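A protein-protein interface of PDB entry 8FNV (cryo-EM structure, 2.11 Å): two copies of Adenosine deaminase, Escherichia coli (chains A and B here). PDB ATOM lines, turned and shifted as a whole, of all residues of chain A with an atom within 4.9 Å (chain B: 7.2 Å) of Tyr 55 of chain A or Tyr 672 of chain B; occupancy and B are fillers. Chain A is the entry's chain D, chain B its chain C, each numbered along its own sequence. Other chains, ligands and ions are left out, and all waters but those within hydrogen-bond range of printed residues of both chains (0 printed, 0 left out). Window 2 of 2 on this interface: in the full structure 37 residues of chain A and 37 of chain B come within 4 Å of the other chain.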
ATOM      1  N   SER A  51      27.750   9.730 -19.242  1.00  0.00           N
ATOM      2  CA  SER A  51      28.156  11.036 -18.730  1.00  0.00           C
ATOM      3  C   SER A  51      29.064  11.764 -19.714  1.00  0.00           C
ATOM      4  O   SER A  51      28.939  12.982 -19.899  1.00  0.00           O
ATOM      5  CB  SER A  51      28.850  10.870 -17.379  1.00  0.00           C
ATOM      6  OG  SER A  51      27.927  10.494 -16.374  1.00  0.00           O
ATOM      7  N   ALA A  52      30.001  11.047 -20.336  1.00  0.00           N
ATOM      8  CA  ALA A  52      30.888  11.676 -21.307  1.00  0.00           C
ATOM      9  C   ALA A  52      30.101  12.218 -22.491  1.00  0.00           C
ATOM     10  O   ALA A  52      30.354  13.335 -22.960  1.00  0.00           O
ATOM     11  CB  ALA A  52      31.945  10.677 -21.775  1.00  0.00           C
ATOM     12  N   TRP A  53      29.134  11.443 -22.986  1.00  0.00           N
ATOM     13  CA  TRP A  53      28.305  11.929 -24.083  1.00  0.00           C
ATOM     14  C   TRP A  53      27.487  13.144 -23.666  1.00  0.00           C
ATOM     15  O   TRP A  53      27.327  14.086 -24.455  1.00  0.00           O
ATOM     16  CB  TRP A  53      27.383  10.820 -24.579  1.00  0.00           C
ATOM     17  CG  TRP A  53      26.476  11.276 -25.665  1.00  0.00           C
ATOM     18  CD1 TRP A  53      25.159  11.607 -25.552  1.00  0.00           C
ATOM     19  CD2 TRP A  53      26.826  11.475 -27.036  1.00  0.00           C
ATOM     20  NE1 TRP A  53      24.663  11.992 -26.773  1.00  0.00           N
ATOM     21  CE2 TRP A  53      25.667  11.920 -27.701  1.00  0.00           C
ATOM     22  CE3 TRP A  53      28.004  11.316 -27.767  1.00  0.00           C
ATOM     23  CZ2 TRP A  53      25.656  12.206 -29.061  1.00  0.00           C
ATOM     24  CZ3 TRP A  53      27.990  11.601 -29.113  1.00  0.00           C
ATOM     25  CH2 TRP A  53      26.825  12.040 -29.747  1.00  0.00           C
ATOM     26  N   SER A  54      26.954  13.132 -22.442  1.00  0.00           N
ATOM     27  CA  SER A  54      26.206  14.286 -21.952  1.00  0.00           C
ATOM     28  C   SER A  54      27.088  15.527 -21.905  1.00  0.00           C
ATOM     29  O   SER A  54      26.666  16.615 -22.312  1.00  0.00           O
ATOM     30  CB  SER A  54      25.627  13.985 -20.572  1.00  0.00           C
ATOM     31  OG  SER A  54      24.430  13.236 -20.676  1.00  0.00           O
ATOM     32  N   TYR A  55      28.321  15.382 -21.417  1.00  0.00           N
ATOM     33  CA  TYR A  55      29.234  16.518 -21.388  1.00  0.00           C
ATOM     34  C   TYR A  55      29.557  16.999 -22.796  1.00  0.00           C
ATOM     35  O   TYR A  55      29.692  18.205 -23.031  1.00  0.00           O
ATOM     36  CB  TYR A  55      30.514  16.150 -20.642  1.00  0.00           C
ATOM     37  CG  TYR A  55      31.427  17.328 -20.401  1.00  0.00           C
ATOM     38  CD1 TYR A  55      31.025  18.388 -19.602  1.00  0.00           C
ATOM     39  CD2 TYR A  55      32.688  17.385 -20.976  1.00  0.00           C
ATOM     40  CE1 TYR A  55      31.854  19.469 -19.380  1.00  0.00           C
ATOM     41  CE2 TYR A  55      33.523  18.461 -20.759  1.00  0.00           C
ATOM     42  CZ  TYR A  55      33.101  19.501 -19.960  1.00  0.00           C
ATOM     43  OH  TYR A  55      33.930  20.576 -19.743  1.00  0.00           O
ATOM     44  N   LEU A  56      29.695  16.073 -23.745  1.00  0.00           N
ATOM     45  CA  LEU A  56      29.987  16.464 -25.121  1.00  0.00           C
ATOM     46  C   LEU A  56      28.847  17.291 -25.712  1.00  0.00           C
ATOM     47  O   LEU A  56      29.076  18.353 -26.310  1.00  0.00           O
ATOM     48  CB  LEU A  56      30.257  15.217 -25.965  1.00  0.00           C
ATOM     49  CG  LEU A  56      30.666  15.430 -27.424  1.00  0.00           C
ATOM     50  CD1 LEU A  56      31.874  16.344 -27.521  1.00  0.00           C
ATOM     51  CD2 LEU A  56      30.957  14.097 -28.091  1.00  0.00           C
ATOM     52  N   VAL A  57      27.606  16.818 -25.554  1.00  0.00           N
ATOM     53  CA  VAL A  57      26.469  17.595 -26.050  1.00  0.00           C
ATOM     54  C   VAL A  57      26.404  18.939 -25.341  1.00  0.00           C
ATOM     55  O   VAL A  57      26.071  19.961 -25.952  1.00  0.00           O
ATOM     56  CB  VAL A  57      25.132  16.839 -25.895  1.00  0.00           C
ATOM     57  CG1 VAL A  57      24.953  15.805 -26.992  1.00  0.00           C
ATOM     58  CG2 VAL A  57      24.973  16.238 -24.511  1.00  0.00           C
ATOM     59  N   GLN A  58      26.694  18.958 -24.039  1.00  0.00           N
ATOM     60  CA  GLN A  58      26.659  20.209 -23.292  1.00  0.00           C
ATOM     61  C   GLN A  58      27.661  21.209 -23.852  1.00  0.00           C
ATOM     62  O   GLN A  58      27.338  22.386 -24.042  1.00  0.00           O
ATOM     63  CB  GLN A  58      26.936  19.925 -21.816  1.00  0.00           C
ATOM     64  CG  GLN A  58      26.825  21.124 -20.900  1.00  0.00           C
ATOM     65  CD  GLN A  58      27.279  20.805 -19.493  1.00  0.00           C
ATOM     66  OE1 GLN A  58      26.549  20.185 -18.722  1.00  0.00           O
ATOM     67  NE2 GLN A  58      28.496  21.211 -19.156  1.00  0.00           N
ATOM     68  N   GLN A  59      28.885  20.754 -24.131  1.00  0.00           N
ATOM     69  CA  GLN A  59      29.890  21.639 -24.710  1.00  0.00           C
ATOM     70  C   GLN A  59      29.443  22.159 -26.069  1.00  0.00           C
ATOM     71  O   GLN A  59      29.538  23.362 -26.348  1.00  0.00           O
ATOM     72  CB  GLN A  59      31.223  20.902 -24.842  1.00  0.00           C
ATOM     73  CG  GLN A  59      31.854  20.501 -23.525  1.00  0.00           C
ATOM     74  CD  GLN A  59      33.055  19.596 -23.715  1.00  0.00           C
ATOM     75  OE1 GLN A  59      32.913  18.386 -23.891  1.00  0.00           O
ATOM     76  NE2 GLN A  59      34.246  20.179 -23.676  1.00  0.00           N
ATOM     77  N   LEU B 549      36.738  12.202 -16.286  1.00  0.00           N
ATOM     78  CA  LEU B 549      35.385  11.697 -16.101  1.00  0.00           C
ATOM     79  C   LEU B 549      34.447  12.867 -15.851  1.00  0.00           C
ATOM     80  O   LEU B 549      34.761  13.763 -15.065  1.00  0.00           O
ATOM     81  CB  LEU B 549      35.312  10.717 -14.930  1.00  0.00           C
ATOM     82  CG  LEU B 549      36.197   9.474 -15.003  1.00  0.00           C
ATOM     83  CD1 LEU B 549      36.267   8.827 -13.636  1.00  0.00           C
ATOM     84  CD2 LEU B 549      35.678   8.494 -16.039  1.00  0.00           C
ATOM     85  N   SER B 550      33.298  12.860 -16.513  1.00  0.00           N
ATOM     86  CA  SER B 550      32.330  13.937 -16.375  1.00  0.00           C
ATOM     87  C   SER B 550      31.259  13.542 -15.368  1.00  0.00           C
ATOM     88  O   SER B 550      30.775  12.406 -15.375  1.00  0.00           O
ATOM     89  CB  SER B 550      31.692  14.276 -17.721  1.00  0.00           C
ATOM     90  OG  SER B 550      30.597  13.429 -17.994  1.00  0.00           O
ATOM     91  N   MET B 551      30.905  14.481 -14.498  1.00  0.00           N
ATOM     92  CA  MET B 551      29.887  14.271 -13.480  1.00  0.00           C
ATOM     93  C   MET B 551      28.919  15.443 -13.520  1.00  0.00           C
ATOM     94  O   MET B 551      29.077  16.375 -14.310  1.00  0.00           O
ATOM     95  CB  MET B 551      30.506  14.157 -12.084  1.00  0.00           C
ATOM     96  CG  MET B 551      31.368  15.365 -11.726  1.00  0.00           C
ATOM     97  SD  MET B 551      32.253  15.326 -10.154  1.00  0.00           S
ATOM     98  CE  MET B 551      32.827  13.645 -10.088  1.00  0.00           C
ATOM     99  N   THR B 552      27.914  15.396 -12.653  1.00  0.00           N
ATOM    100  CA  THR B 552      27.026  16.534 -12.479  1.00  0.00           C
ATOM    101  C   THR B 552      27.623  17.524 -11.485  1.00  0.00           C
ATOM    102  O   THR B 552      28.420  17.164 -10.615  1.00  0.00           O
ATOM    103  CB  THR B 552      25.646  16.081 -12.004  1.00  0.00           C
ATOM    104  OG1 THR B 552      25.768  15.371 -10.766  1.00  0.00           O
ATOM    105  CG2 THR B 552      24.991  15.190 -13.045  1.00  0.00           C
ATOM    106  N   LYS B 553      27.231  18.790 -11.634  1.00  0.00           N
ATOM    107  CA  LYS B 553      27.771  19.836 -10.771  1.00  0.00           C
ATOM    108  C   LYS B 553      27.393  19.614  -9.314  1.00  0.00           C
ATOM    109  O   LYS B 553      28.180  19.932  -8.417  1.00  0.00           O
ATOM    110  CB  LYS B 553      27.290  21.207 -11.242  1.00  0.00           C
ATOM    111  CG  LYS B 553      27.884  21.630 -12.571  1.00  0.00           C
ATOM    112  CD  LYS B 553      28.023  23.137 -12.682  1.00  0.00           C
ATOM    113  CE  LYS B 553      28.767  23.522 -13.950  1.00  0.00           C
ATOM    114  NZ  LYS B 553      28.021  24.440 -14.853  1.00  0.00           N
ATOM    115  N   LYS B 667      18.856  23.511 -12.998  1.00  0.00           N
ATOM    116  CA  LYS B 667      19.525  23.338 -14.283  1.00  0.00           C
ATOM    117  C   LYS B 667      21.036  23.244 -14.103  1.00  0.00           C
ATOM    118  O   LYS B 667      21.691  22.386 -14.709  1.00  0.00           O
ATOM    119  CB  LYS B 667      19.161  24.492 -15.219  1.00  0.00           C
ATOM    120  CG  LYS B 667      19.514  24.253 -16.684  1.00  0.00           C
ATOM    121  CD  LYS B 667      19.424  25.532 -17.519  1.00  0.00           C
ATOM    122  CE  LYS B 667      20.367  26.626 -17.031  1.00  0.00           C
ATOM    123  NZ  LYS B 667      21.678  26.097 -16.564  1.00  0.00           N
ATOM    124  N   GLN B 668      21.608  24.108 -13.262  1.00  0.00           N
ATOM    125  CA  GLN B 668      23.040  24.040 -12.998  1.00  0.00           C
ATOM    126  C   GLN B 668      23.423  22.750 -12.282  1.00  0.00           C
ATOM    127  O   GLN B 668      24.527  22.237 -12.487  1.00  0.00           O
ATOM    128  CB  GLN B 668      23.477  25.255 -12.182  1.00  0.00           C
ATOM    129  CG  GLN B 668      23.807  26.466 -13.038  1.00  0.00           C
ATOM    130  CD  GLN B 668      25.205  26.410 -13.620  1.00  0.00           C
ATOM    131  OE1 GLN B 668      26.076  25.706 -13.112  1.00  0.00           O
ATOM    132  NE2 GLN B 668      25.421  27.146 -14.703  1.00  0.00           N
ATOM    133  N   ARG B 669      22.537  22.224 -11.436  1.00  0.00           N
ATOM    134  CA  ARG B 669      22.793  20.947 -10.779  1.00  0.00           C
ATOM    135  C   ARG B 669      22.859  19.819 -11.796  1.00  0.00           C
ATOM    136  O   ARG B 669      23.723  18.940 -11.706  1.00  0.00           O
ATOM    137  CB  ARG B 669      21.700  20.669  -9.746  1.00  0.00           C
ATOM    138  CG  ARG B 669      21.972  21.259  -8.373  1.00  0.00           C
ATOM    139  CD  ARG B 669      20.763  21.148  -7.458  1.00  0.00           C
ATOM    140  NE  ARG B 669      20.475  19.778  -7.047  1.00  0.00           N
ATOM    141  CZ  ARG B 669      19.488  19.442  -6.227  1.00  0.00           C
ATOM    142  NH1 ARG B 669      18.670  20.350  -5.722  1.00  0.00           N
ATOM    143  NH2 ARG B 669      19.320  18.162  -5.905  1.00  0.00           N
ATOM    144  N   ALA B 670      21.953  19.829 -12.773  1.00  0.00           N
ATOM    145  CA  ALA B 670      21.968  18.807 -13.812  1.00  0.00           C
ATOM    146  C   ALA B 670      23.080  19.019 -14.832  1.00  0.00           C
ATOM    147  O   ALA B 670      23.410  18.084 -15.568  1.00  0.00           O
ATOM    148  CB  ALA B 670      20.616  18.756 -14.524  1.00  0.00           C
ATOM    149  N   GLU B 671      23.655  20.218 -14.897  1.00  0.00           N
ATOM    150  CA  GLU B 671      24.801  20.456 -15.765  1.00  0.00           C
ATOM    151  C   GLU B 671      25.919  19.458 -15.472  1.00  0.00           C
ATOM    152  O   GLU B 671      25.955  18.815 -14.420  1.00  0.00           O
ATOM    153  CB  GLU B 671      25.332  21.876 -15.581  1.00  0.00           C
ATOM    154  CG  GLU B 671      24.517  22.940 -16.276  1.00  0.00           C
ATOM    155  CD  GLU B 671      24.703  22.931 -17.780  1.00  0.00           C
ATOM    156  OE1 GLU B 671      25.805  23.292 -18.240  1.00  0.00           O
ATOM    157  OE2 GLU B 671      23.749  22.567 -18.500  1.00  0.00           O
ATOM    158  N   TYR B 672      26.847  19.343 -16.420  1.00  0.00           N
ATOM    159  CA  TYR B 672      27.972  18.425 -16.316  1.00  0.00           C
ATOM    160  C   TYR B 672      29.289  19.190 -16.339  1.00  0.00           C
ATOM    161  O   TYR B 672      29.407  20.232 -16.990  1.00  0.00           O
ATOM    162  CB  TYR B 672      27.959  17.396 -17.450  1.00  0.00           C
ATOM    163  CG  TYR B 672      26.909  16.322 -17.290  1.00  0.00           C
ATOM    164  CD1 TYR B 672      25.605  16.533 -17.713  1.00  0.00           C
ATOM    165  CD2 TYR B 672      27.218  15.105 -16.703  1.00  0.00           C
ATOM    166  CE1 TYR B 672      24.642  15.557 -17.566  1.00  0.00           C
ATOM    167  CE2 TYR B 672      26.261  14.124 -16.550  1.00  0.00           C
ATOM    168  CZ  TYR B 672      24.974  14.355 -16.983  1.00  0.00           C
ATOM    169  OH  TYR B 672      24.017  13.379 -16.833  1.00  0.00           O
ATOM    170  N   VAL B 673      30.277  18.661 -15.617  1.00  0.00           N
ATOM    171  CA  VAL B 673      31.618  19.224 -15.561  1.00  0.00           C
ATOM    172  C   VAL B 673      32.608  18.069 -15.499  1.00  0.00           C
ATOM    173  O   VAL B 673      32.305  16.991 -14.978  1.00  0.00           O
ATOM    174  CB  VAL B 673      31.793  20.173 -14.348  1.00  0.00           C
ATOM    175  CG1 VAL B 673      31.382  19.502 -13.047  1.00  0.00           C
ATOM    176  CG2 VAL B 673      33.196  20.783 -14.272  1.00  0.00           C
ATOM    177  N   GLU B 674      33.803  18.301 -16.033  1.00  0.00           N
ATOM    178  CA  GLU B 674      34.833  17.274 -16.119  1.00  0.00           C
ATOM    179  C   GLU B 674      35.754  17.338 -14.908  1.00  0.00           C
ATOM    180  O   GLU B 674      36.077  18.424 -14.415  1.00  0.00           O
ATOM    181  CB  GLU B 674      35.648  17.432 -17.403  1.00  0.00           C
ATOM    182  CG  GLU B 674      35.288  16.431 -18.487  1.00  0.00           C
ATOM    183  CD  GLU B 674      36.262  16.454 -19.650  1.00  0.00           C
ATOM    184  OE1 GLU B 674      37.412  16.905 -19.458  1.00  0.00           O
ATOM    185  OE2 GLU B 674      35.879  16.020 -20.756  1.00  0.00           O
ATOM    186  N   VAL B 675      36.174  16.167 -14.435  1.00  0.00           N
ATOM    187  CA  VAL B 675      37.102  16.029 -13.322  1.00  0.00           C
ATOM    188  C   VAL B 675      38.201  15.068 -13.746  1.00  0.00           C
ATOM    189  O   VAL B 675      37.924  14.010 -14.323  1.00  0.00           O
ATOM    190  CB  VAL B 675      36.395  15.516 -12.050  1.00  0.00           C
ATOM    191  CG1 VAL B 675      37.398  15.217 -10.937  1.00  0.00           C
ATOM    192  CG2 VAL B 675      35.319  16.489 -11.594  1.00  0.00           C
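The backbone NH (N) of Val 673 of chain B sits at hydrogen-bond distance from the backbone carbonyl oxygen (O) of Met 551 of chain B (2.9 Å).
N of Lys 553 of chain B sits at hydrogen-bond distance from O of Glu 671 of chain B, at 3.1 Å.
O of Tyr 55 of chain A lies close to OE1 of Gln 59 of chain A, at 3.3 Å.
Among the printed residues, pairs that only touch across the chains: Ser 51 of chain A with Tyr 672 of chain B (3.998 Å), Ser 54 of chain A with Tyr 672 of chain B (3.5 Å), Tyr 55 of chain A with Ser 550 of chain B (3.7 Å), Tyr 55 of chain A with Tyr 672 of chain B (3.5 Å), Tyr 55 of chain A with Val 673 of chain B (3.8 Å) and Tyr 55 of chain A with Glu 674 of chain B (3.4 Å).
The backbone carbonyl oxygen of Ser 51 of chain A lies within hydrogen-bond range of the side-chain hydroxyl of Ser 550 of chain B (2.6 Å).
The side-chain hydroxyl (OG) of Ser 550 of chain B sits at hydrogen-bond distance from the backbone NH (N) of Ala 52 of chain A.
OE1 of Glu 671 of chain B lies close to OE1 of Gln 58 of chain A, 3.2 Å away.
N of Tyr 672 of chain B sits at hydrogen-bond distance from OE1 of Gln 58 of chain A (2.5 Å).
No position is printed for both chains.
Of the 14 printed residues of chain B, 5 touch a printed residue of chain A.
Hydrophobic or aromatic side chains of chain B within 4 Å of the printed part of chain A: Tyr 672.
Of the printed residues of chain B, Ser 51 of chain A touches Ser 550 and Tyr 672.
Of the printed residues of chain B, Ala 52 of chain A touches Ser 550 (3.4 Å).
Of the printed residues of chain B, Ser 54 of chain A touches Tyr 672.
Tyr 55 of chain A touches just these residues of chain B: Ser 550, Tyr 672, Val 673 and Glu 674.
Leu 56 of chain A touches none of the printed residues of chain B.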
